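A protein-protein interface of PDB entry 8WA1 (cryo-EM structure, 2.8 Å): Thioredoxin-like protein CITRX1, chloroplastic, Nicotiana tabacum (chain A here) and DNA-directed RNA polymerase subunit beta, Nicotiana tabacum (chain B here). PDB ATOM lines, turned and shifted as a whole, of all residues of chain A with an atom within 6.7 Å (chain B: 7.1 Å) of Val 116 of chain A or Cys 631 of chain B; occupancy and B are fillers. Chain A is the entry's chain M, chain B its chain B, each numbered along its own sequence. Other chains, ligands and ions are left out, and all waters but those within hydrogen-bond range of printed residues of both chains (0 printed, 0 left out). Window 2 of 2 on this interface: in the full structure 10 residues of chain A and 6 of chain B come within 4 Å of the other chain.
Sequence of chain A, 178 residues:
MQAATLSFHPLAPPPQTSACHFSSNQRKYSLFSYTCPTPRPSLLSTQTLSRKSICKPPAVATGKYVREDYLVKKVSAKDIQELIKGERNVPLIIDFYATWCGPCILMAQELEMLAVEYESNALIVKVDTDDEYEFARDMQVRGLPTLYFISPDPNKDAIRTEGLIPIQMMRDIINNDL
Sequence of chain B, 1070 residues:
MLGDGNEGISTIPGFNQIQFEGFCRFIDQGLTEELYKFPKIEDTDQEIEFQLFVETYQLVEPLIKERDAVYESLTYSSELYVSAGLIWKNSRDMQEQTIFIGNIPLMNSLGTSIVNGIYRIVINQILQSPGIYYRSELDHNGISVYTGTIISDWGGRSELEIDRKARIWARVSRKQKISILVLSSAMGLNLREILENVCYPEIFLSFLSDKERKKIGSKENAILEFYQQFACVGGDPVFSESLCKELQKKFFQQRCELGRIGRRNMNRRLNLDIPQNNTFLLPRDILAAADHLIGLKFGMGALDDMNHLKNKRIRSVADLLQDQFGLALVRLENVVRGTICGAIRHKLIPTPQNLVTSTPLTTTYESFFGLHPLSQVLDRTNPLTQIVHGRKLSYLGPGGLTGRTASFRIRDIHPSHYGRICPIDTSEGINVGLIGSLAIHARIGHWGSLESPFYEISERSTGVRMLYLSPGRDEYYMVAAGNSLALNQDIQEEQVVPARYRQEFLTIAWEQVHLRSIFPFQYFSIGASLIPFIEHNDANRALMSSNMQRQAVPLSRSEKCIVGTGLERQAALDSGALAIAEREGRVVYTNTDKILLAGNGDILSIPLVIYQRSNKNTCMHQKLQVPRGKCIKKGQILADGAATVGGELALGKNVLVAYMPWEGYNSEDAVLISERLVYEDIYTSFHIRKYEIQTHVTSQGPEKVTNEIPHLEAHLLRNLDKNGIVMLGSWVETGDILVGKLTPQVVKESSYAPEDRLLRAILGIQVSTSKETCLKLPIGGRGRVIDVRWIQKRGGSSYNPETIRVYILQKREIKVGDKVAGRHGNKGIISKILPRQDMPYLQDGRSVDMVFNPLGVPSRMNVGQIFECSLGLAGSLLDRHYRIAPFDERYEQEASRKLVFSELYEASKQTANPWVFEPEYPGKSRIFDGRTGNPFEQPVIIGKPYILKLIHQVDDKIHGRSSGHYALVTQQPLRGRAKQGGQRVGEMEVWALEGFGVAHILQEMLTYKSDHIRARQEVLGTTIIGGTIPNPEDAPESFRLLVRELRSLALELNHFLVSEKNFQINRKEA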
ATOM      1  N   LEU A  71     -15.795 -11.335  -5.031  1.00  0.00           N
ATOM      2  CA  LEU A  71     -15.372 -12.250  -6.084  1.00  0.00           C
ATOM      3  C   LEU A  71     -16.217 -13.515  -6.163  1.00  0.00           C
ATOM      4  O   LEU A  71     -15.989 -14.338  -7.055  1.00  0.00           O
ATOM      5  CB  LEU A  71     -13.899 -12.632  -5.893  1.00  0.00           C
ATOM      6  CG  LEU A  71     -12.826 -11.684  -6.438  1.00  0.00           C
ATOM      7  CD1 LEU A  71     -12.790 -10.365  -5.679  1.00  0.00           C
ATOM      8  CD2 LEU A  71     -11.464 -12.361  -6.405  1.00  0.00           C
ATOM      9  N   LEU A 111     -15.033 -17.329   2.960  1.00  0.00           N
ATOM     10  CA  LEU A 111     -15.128 -17.735   1.561  1.00  0.00           C
ATOM     11  C   LEU A 111     -14.487 -16.701   0.646  1.00  0.00           C
ATOM     12  O   LEU A 111     -13.860 -17.057  -0.356  1.00  0.00           O
ATOM     13  CB  LEU A 111     -16.587 -17.970   1.175  1.00  0.00           C
ATOM     14  CG  LEU A 111     -17.094 -19.416   1.232  1.00  0.00           C
ATOM     15  CD1 LEU A 111     -16.307 -20.297   0.280  1.00  0.00           C
ATOM     16  CD2 LEU A 111     -17.018 -19.972   2.639  1.00  0.00           C
ATOM     17  N   GLU A 112     -14.632 -15.414   0.973  1.00  0.00           N
ATOM     18  CA  GLU A 112     -13.931 -14.374   0.226  1.00  0.00           C
ATOM     19  C   GLU A 112     -12.422 -14.548   0.328  1.00  0.00           C
ATOM     20  O   GLU A 112     -11.707 -14.462  -0.680  1.00  0.00           O
ATOM     21  CB  GLU A 112     -14.341 -12.993   0.733  1.00  0.00           C
ATOM     22  CG  GLU A 112     -15.726 -12.543   0.308  1.00  0.00           C
ATOM     23  CD  GLU A 112     -15.800 -12.201  -1.166  1.00  0.00           C
ATOM     24  OE1 GLU A 112     -16.287 -13.040  -1.951  1.00  0.00           O
ATOM     25  OE2 GLU A 112     -15.360 -11.094  -1.541  1.00  0.00           O
ATOM     26  N   MET A 113     -11.917 -14.786   1.541  1.00  0.00           N
ATOM     27  CA  MET A 113     -10.484 -15.016   1.711  1.00  0.00           C
ATOM     28  C   MET A 113     -10.018 -16.238   0.932  1.00  0.00           C
ATOM     29  O   MET A 113      -8.941 -16.216   0.325  1.00  0.00           O
ATOM     30  CB  MET A 113     -10.139 -15.180   3.191  1.00  0.00           C
ATOM     31  CG  MET A 113      -9.869 -13.879   3.923  1.00  0.00           C
ATOM     32  SD  MET A 113      -8.507 -12.941   3.201  1.00  0.00           S
ATOM     33  CE  MET A 113      -7.149 -14.093   3.397  1.00  0.00           C
ATOM     34  N   LEU A 114     -10.816 -17.307   0.932  1.00  0.00           N
ATOM     35  CA  LEU A 114     -10.440 -18.518   0.212  1.00  0.00           C
ATOM     36  C   LEU A 114     -10.444 -18.287  -1.293  1.00  0.00           C
ATOM     37  O   LEU A 114      -9.581 -18.805  -2.012  1.00  0.00           O
ATOM     38  CB  LEU A 114     -11.389 -19.655   0.589  1.00  0.00           C
ATOM     39  CG  LEU A 114     -11.024 -21.059   0.111  1.00  0.00           C
ATOM     40  CD1 LEU A 114      -9.726 -21.514   0.754  1.00  0.00           C
ATOM     41  CD2 LEU A 114     -12.151 -22.031   0.420  1.00  0.00           C
ATOM     42  N   ALA A 115     -11.413 -17.513  -1.788  1.00  0.00           N
ATOM     43  CA  ALA A 115     -11.457 -17.191  -3.210  1.00  0.00           C
ATOM     44  C   ALA A 115     -10.276 -16.320  -3.612  1.00  0.00           C
ATOM     45  O   ALA A 115      -9.757 -16.441  -4.727  1.00  0.00           O
ATOM     46  CB  ALA A 115     -12.778 -16.500  -3.551  1.00  0.00           C
ATOM     47  N   VAL A 116      -9.846 -15.424  -2.721  1.00  0.00           N
ATOM     48  CA  VAL A 116      -8.654 -14.629  -3.000  1.00  0.00           C
ATOM     49  C   VAL A 116      -7.415 -15.517  -3.014  1.00  0.00           C
ATOM     50  O   VAL A 116      -6.535 -15.366  -3.871  1.00  0.00           O
ATOM     51  CB  VAL A 116      -8.522 -13.480  -1.982  1.00  0.00           C
ATOM     52  CG1 VAL A 116      -7.213 -12.741  -2.183  1.00  0.00           C
ATOM     53  CG2 VAL A 116      -9.691 -12.517  -2.118  1.00  0.00           C
ATOM     54  N   GLU A 117      -7.331 -16.462  -2.073  1.00  0.00           N
ATOM     55  CA  GLU A 117      -6.175 -17.352  -2.020  1.00  0.00           C
ATOM     56  C   GLU A 117      -6.137 -18.294  -3.218  1.00  0.00           C
ATOM     57  O   GLU A 117      -5.056 -18.658  -3.693  1.00  0.00           O
ATOM     58  CB  GLU A 117      -6.179 -18.145  -0.711  1.00  0.00           C
ATOM     59  CG  GLU A 117      -5.916 -17.303   0.526  1.00  0.00           C
ATOM     60  CD  GLU A 117      -5.755 -18.137   1.781  1.00  0.00           C
ATOM     61  OE1 GLU A 117      -5.791 -19.382   1.678  1.00  0.00           O
ATOM     62  OE2 GLU A 117      -5.592 -17.547   2.869  1.00  0.00           O
ATOM     63  N   TYR A 118      -7.302 -18.694  -3.723  1.00  0.00           N
ATOM     64  CA  TYR A 118      -7.413 -19.571  -4.889  1.00  0.00           C
ATOM     65  C   TYR A 118      -8.031 -18.755  -6.021  1.00  0.00           C
ATOM     66  O   TYR A 118      -9.250 -18.756  -6.213  1.00  0.00           O
ATOM     67  CB  TYR A 118      -8.246 -20.823  -4.564  1.00  0.00           C
ATOM     68  CG  TYR A 118      -7.561 -21.798  -3.633  1.00  0.00           C
ATOM     69  CD1 TYR A 118      -7.598 -21.619  -2.256  1.00  0.00           C
ATOM     70  CD2 TYR A 118      -6.878 -22.899  -4.131  1.00  0.00           C
ATOM     71  CE1 TYR A 118      -6.973 -22.508  -1.402  1.00  0.00           C
ATOM     72  CE2 TYR A 118      -6.251 -23.794  -3.285  1.00  0.00           C
ATOM     73  CZ  TYR A 118      -6.301 -23.595  -1.923  1.00  0.00           C
ATOM     74  OH  TYR A 118      -5.676 -24.484  -1.079  1.00  0.00           O
ATOM     75  N   GLU A 119      -7.177 -18.064  -6.777  1.00  0.00           N
ATOM     76  CA  GLU A 119      -7.665 -17.148  -7.804  1.00  0.00           C
ATOM     77  C   GLU A 119      -8.353 -17.899  -8.940  1.00  0.00           C
ATOM     78  O   GLU A 119      -9.505 -17.605  -9.281  1.00  0.00           O
ATOM     79  CB  GLU A 119      -6.517 -16.284  -8.336  1.00  0.00           C
ATOM     80  CG  GLU A 119      -5.219 -17.031  -8.619  1.00  0.00           C
ATOM     81  CD  GLU A 119      -4.327 -17.151  -7.398  1.00  0.00           C
ATOM     82  OE1 GLU A 119      -4.684 -16.593  -6.339  1.00  0.00           O
ATOM     83  OE2 GLU A 119      -3.268 -17.805  -7.498  1.00  0.00           O
ATOM     84  N   ILE A 124     -15.658 -21.016  -6.705  1.00  0.00           N
ATOM     85  CA  ILE A 124     -16.454 -20.811  -5.501  1.00  0.00           C
ATOM     86  C   ILE A 124     -17.717 -20.051  -5.881  1.00  0.00           C
ATOM     87  O   ILE A 124     -17.641 -18.948  -6.433  1.00  0.00           O
ATOM     88  CB  ILE A 124     -15.667 -20.052  -4.419  1.00  0.00           C
ATOM     89  CG1 ILE A 124     -14.474 -20.882  -3.943  1.00  0.00           C
ATOM     90  CG2 ILE A 124     -16.575 -19.695  -3.257  1.00  0.00           C
ATOM     91  CD1 ILE A 124     -13.669 -20.222  -2.845  1.00  0.00           C
ATOM     92  N   GLU B 584      -7.455  -7.161  -5.328  1.00  0.00           N
ATOM     93  CA  GLU B 584      -7.081  -8.358  -4.594  1.00  0.00           C
ATOM     94  C   GLU B 584      -5.871  -9.024  -5.245  1.00  0.00           C
ATOM     95  O   GLU B 584      -5.645  -8.922  -6.454  1.00  0.00           O
ATOM     96  CB  GLU B 584      -8.251  -9.342  -4.523  1.00  0.00           C
ATOM     97  CG  GLU B 584      -8.640  -9.968  -5.856  1.00  0.00           C
ATOM     98  CD  GLU B 584      -9.440  -9.029  -6.738  1.00  0.00           C
ATOM     99  OE1 GLU B 584      -9.891  -7.978  -6.237  1.00  0.00           O
ATOM    100  OE2 GLU B 584      -9.616  -9.342  -7.934  1.00  0.00           O
ATOM    101  N   GLY B 585      -5.087  -9.705  -4.423  1.00  0.00           N
ATOM    102  CA  GLY B 585      -3.899 -10.373  -4.909  1.00  0.00           C
ATOM    103  C   GLY B 585      -2.961 -10.705  -3.766  1.00  0.00           C
ATOM    104  O   GLY B 585      -3.332 -10.655  -2.595  1.00  0.00           O
ATOM    105  N   ARG B 586      -1.732 -11.044  -4.142  1.00  0.00           N
ATOM    106  CA  ARG B 586      -0.689 -11.411  -3.197  1.00  0.00           C
ATOM    107  C   ARG B 586       0.476 -10.434  -3.299  1.00  0.00           C
ATOM    108  O   ARG B 586       0.773  -9.905  -4.374  1.00  0.00           O
ATOM    109  CB  ARG B 586      -0.203 -12.841  -3.452  1.00  0.00           C
ATOM    110  CG  ARG B 586       0.609 -13.444  -2.320  1.00  0.00           C
ATOM    111  CD  ARG B 586       0.968 -14.898  -2.600  1.00  0.00           C
ATOM    112  NE  ARG B 586      -0.206 -15.767  -2.645  1.00  0.00           N
ATOM    113  CZ  ARG B 586      -0.800 -16.169  -3.765  1.00  0.00           C
ATOM    114  NH1 ARG B 586      -0.332 -15.782  -4.944  1.00  0.00           N
ATOM    115  NH2 ARG B 586      -1.863 -16.961  -3.707  1.00  0.00           N
ATOM    116  N   VAL B 587       1.135 -10.199  -2.166  1.00  0.00           N
ATOM    117  CA  VAL B 587       2.258  -9.262  -2.096  1.00  0.00           C
ATOM    118  C   VAL B 587       3.516 -10.068  -2.409  1.00  0.00           C
ATOM    119  O   VAL B 587       4.061 -10.773  -1.559  1.00  0.00           O
ATOM    120  CB  VAL B 587       2.335  -8.558  -0.744  1.00  0.00           C
ATOM    121  CG1 VAL B 587       3.444  -7.524  -0.752  1.00  0.00           C
ATOM    122  CG2 VAL B 587       1.002  -7.911  -0.410  1.00  0.00           C
ATOM    123  N   LEU B 597       2.010  -5.711  -5.676  1.00  0.00           N
ATOM    124  CA  LEU B 597       0.841  -6.543  -5.426  1.00  0.00           C
ATOM    125  C   LEU B 597       0.453  -7.239  -6.723  1.00  0.00           C
ATOM    126  O   LEU B 597       0.050  -6.579  -7.687  1.00  0.00           O
ATOM    127  CB  LEU B 597      -0.322  -5.703  -4.892  1.00  0.00           C
ATOM    128  CG  LEU B 597      -1.608  -6.434  -4.506  1.00  0.00           C
ATOM    129  CD1 LEU B 597      -1.359  -7.385  -3.346  1.00  0.00           C
ATOM    130  CD2 LEU B 597      -2.695  -5.432  -4.156  1.00  0.00           C
ATOM    131  N   VAL B 626       1.645  -5.509   6.201  1.00  0.00           N
ATOM    132  CA  VAL B 626       1.481  -6.887   5.725  1.00  0.00           C
ATOM    133  C   VAL B 626       2.845  -7.465   5.371  1.00  0.00           C
ATOM    134  O   VAL B 626       3.689  -6.749   4.800  1.00  0.00           O
ATOM    135  CB  VAL B 626       0.532  -6.925   4.524  1.00  0.00           C
ATOM    136  CG1 VAL B 626      -0.882  -6.574   4.962  1.00  0.00           C
ATOM    137  CG2 VAL B 626       1.000  -5.965   3.440  1.00  0.00           C
ATOM    138  N   PRO B 627       3.119  -8.722   5.697  1.00  0.00           N
ATOM    139  CA  PRO B 627       4.363  -9.360   5.264  1.00  0.00           C
ATOM    140  C   PRO B 627       4.235  -9.913   3.848  1.00  0.00           C
ATOM    141  O   PRO B 627       3.161  -9.911   3.242  1.00  0.00           O
ATOM    142  CB  PRO B 627       4.543 -10.491   6.282  1.00  0.00           C
ATOM    143  CG  PRO B 627       3.151 -10.852   6.665  1.00  0.00           C
ATOM    144  CD  PRO B 627       2.368  -9.564   6.646  1.00  0.00           C
ATOM    145  N   GLY B 629       3.811 -12.453   0.974  1.00  0.00           N
ATOM    146  CA  GLY B 629       3.200 -13.740   0.718  1.00  0.00           C
ATOM    147  C   GLY B 629       1.818 -13.951   1.296  1.00  0.00           C
ATOM    148  O   GLY B 629       1.346 -15.094   1.315  1.00  0.00           O
ATOM    149  N   LYS B 630       1.153 -12.900   1.764  1.00  0.00           N
ATOM    150  CA  LYS B 630      -0.205 -13.001   2.278  1.00  0.00           C
ATOM    151  C   LYS B 630      -1.176 -12.315   1.326  1.00  0.00           C
ATOM    152  O   LYS B 630      -0.810 -11.366   0.626  1.00  0.00           O
ATOM    153  CB  LYS B 630      -0.323 -12.388   3.676  1.00  0.00           C
ATOM    154  CG  LYS B 630      -0.097 -10.889   3.730  1.00  0.00           C
ATOM    155  CD  LYS B 630      -0.706 -10.299   4.989  1.00  0.00           C
ATOM    156  CE  LYS B 630      -2.214 -10.488   5.011  1.00  0.00           C
ATOM    157  NZ  LYS B 630      -2.831  -9.879   6.220  1.00  0.00           N
ATOM    158  N   CYS B 631      -2.413 -12.805   1.301  1.00  0.00           N
ATOM    159  CA  CYS B 631      -3.428 -12.242   0.424  1.00  0.00           C
ATOM    160  C   CYS B 631      -4.120 -11.056   1.087  1.00  0.00           C
ATOM    161  O   CYS B 631      -4.354 -11.039   2.298  1.00  0.00           O
ATOM    162  CB  CYS B 631      -4.456 -13.307   0.051  1.00  0.00           C
ATOM    163  SG  CYS B 631      -3.758 -14.735  -0.804  1.00  0.00           S
ATOM    164  N   ILE B 632      -4.450 -10.056   0.274  1.00  0.00           N
ATOM    165  CA  ILE B 632      -5.110  -8.840   0.733  1.00  0.00           C
ATOM    166  C   ILE B 632      -6.298  -8.561  -0.176  1.00  0.00           C
ATOM    167  O   ILE B 632      -6.171  -8.593  -1.405  1.00  0.00           O
ATOM    168  CB  ILE B 632      -4.139  -7.636   0.753  1.00  0.00           C
ATOM    169  CG1 ILE B 632      -3.197  -7.714   1.957  1.00  0.00           C
ATOM    170  CG2 ILE B 632      -4.898  -6.322   0.770  1.00  0.00           C
ATOM    171  CD1 ILE B 632      -1.930  -8.490   1.700  1.00  0.00           C
ATOM    172  N   LYS B 633      -7.452  -8.288   0.429  1.00  0.00           N
ATOM    173  CA  LYS B 633      -8.657  -7.978  -0.323  1.00  0.00           C
ATOM    174  C   LYS B 633      -8.625  -6.525  -0.794  1.00  0.00           C
ATOM    175  O   LYS B 633      -7.715  -5.758  -0.479  1.00  0.00           O
ATOM    176  CB  LYS B 633      -9.905  -8.233   0.519  1.00  0.00           C
ATOM    177  CG  LYS B 633     -10.087  -9.662   0.995  1.00  0.00           C
ATOM    178  CD  LYS B 633     -11.416  -9.796   1.720  1.00  0.00           C
ATOM    179  CE  LYS B 633     -11.534 -11.121   2.443  1.00  0.00           C
ATOM    180  NZ  LYS B 633     -12.802 -11.211   3.219  1.00  0.00           N
ATOM    181  N   LYS B 634      -9.643  -6.137  -1.557  1.00  0.00           N
ATOM    182  CA  LYS B 634      -9.771  -4.764  -2.036  1.00  0.00           C
ATOM    183  C   LYS B 634     -10.368  -3.927  -0.912  1.00  0.00           C
ATOM    184  O   LYS B 634     -11.588  -3.872  -0.744  1.00  0.00           O
ATOM    185  CB  LYS B 634     -10.629  -4.705  -3.295  1.00  0.00           C
ATOM    186  CG  LYS B 634     -10.802  -3.303  -3.850  1.00  0.00           C
ATOM    187  CD  LYS B 634     -11.713  -3.290  -5.063  1.00  0.00           C
ATOM    188  CE  LYS B 634     -11.935  -1.872  -5.559  1.00  0.00           C
ATOM    189  NZ  LYS B 634     -12.554  -1.018  -4.510  1.00  0.00           N
ATOM    190  N   GLN B 636      -8.368  -3.622   2.330  1.00  0.00           N
ATOM    191  CA  GLN B 636      -7.565  -3.836   3.521  1.00  0.00           C
ATOM    192  C   GLN B 636      -6.362  -2.892   3.537  1.00  0.00           C
ATOM    193  O   GLN B 636      -6.043  -2.223   2.552  1.00  0.00           O
ATOM    194  CB  GLN B 636      -7.113  -5.293   3.601  1.00  0.00           C
ATOM    195  CG  GLN B 636      -8.262  -6.281   3.701  1.00  0.00           C
ATOM    196  CD  GLN B 636      -7.790  -7.706   3.888  1.00  0.00           C
ATOM    197  OE1 GLN B 636      -8.596  -8.625   4.022  1.00  0.00           O
ATOM    198  NE2 GLN B 636      -6.476  -7.898   3.900  1.00  0.00           N
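Of the 14 printed residues of chain B, 4 touch a printed residue of chain A.
Among the printed residues, 7 pairs touch across the chains.
Among the printed residues, Asp or Glu carboxylates within 4 Å of a Lys or Arg side-chain nitrogen of the other chain: Glu 119 of chain A with Arg 586 of chain B (3.9 Å).
CG of Glu 584 of chain B touches CD2 of Leu 71 of chain A, at 3.7 Å.
Glu 112 of chain A touches Lys 633 of chain B (CB to NZ, 3.4 Å).
Lys 633 of chain B touches Met 113 of chain A.
Cys 631 of chain B touches Val 116 of chain A (CB to CG1, 3.6 Å).
O of Glu 117 of chain A touches NH2 of Arg 586 of chain B, 3.6 Å away.
SG of Cys 631 of chain B touches CG of Glu 117 of chain A (3.6 Å).
Of the printed residues of chain B, Leu 71 of chain A touches Glu 584.
Val 116 of chain A touches one residue of chain B.
Printed residues of chain B within 4 Å of Glu 117 of chain A: Arg 586 (3.6 Å) and Cys 631 (3.6 Å).
Tyr 118 of chain A touches none of the printed residues of chain B.
Of the printed residues of chain B, Glu 119 of chain A touches Arg 586 (3.9 Å).
Of the printed residues of chain A, Glu 584 of chain B touches Leu 71.
Of chain A, only Val 116 and Glu 117 come within 4 Å of Cys 631 of chain B.
The nearest printed residue of chain B that does not touch Val 116 of chain A is Glu 584 of chain B (4.2 Å).
The nearest residue of chain A that does not touch Cys 631 of chain B is Met 113 of chain A (4.3 Å).
The nearest printed residue of chain A that does not touch Glu 584 of chain B is Val 116 of chain A (4.2 Å).
The side-chain carboxylate (OE1) of Glu 119 of chain A lies within salt-bridge range of the guanidinium group (NH2) of Arg 586 of chain B, 3.9 Å away.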
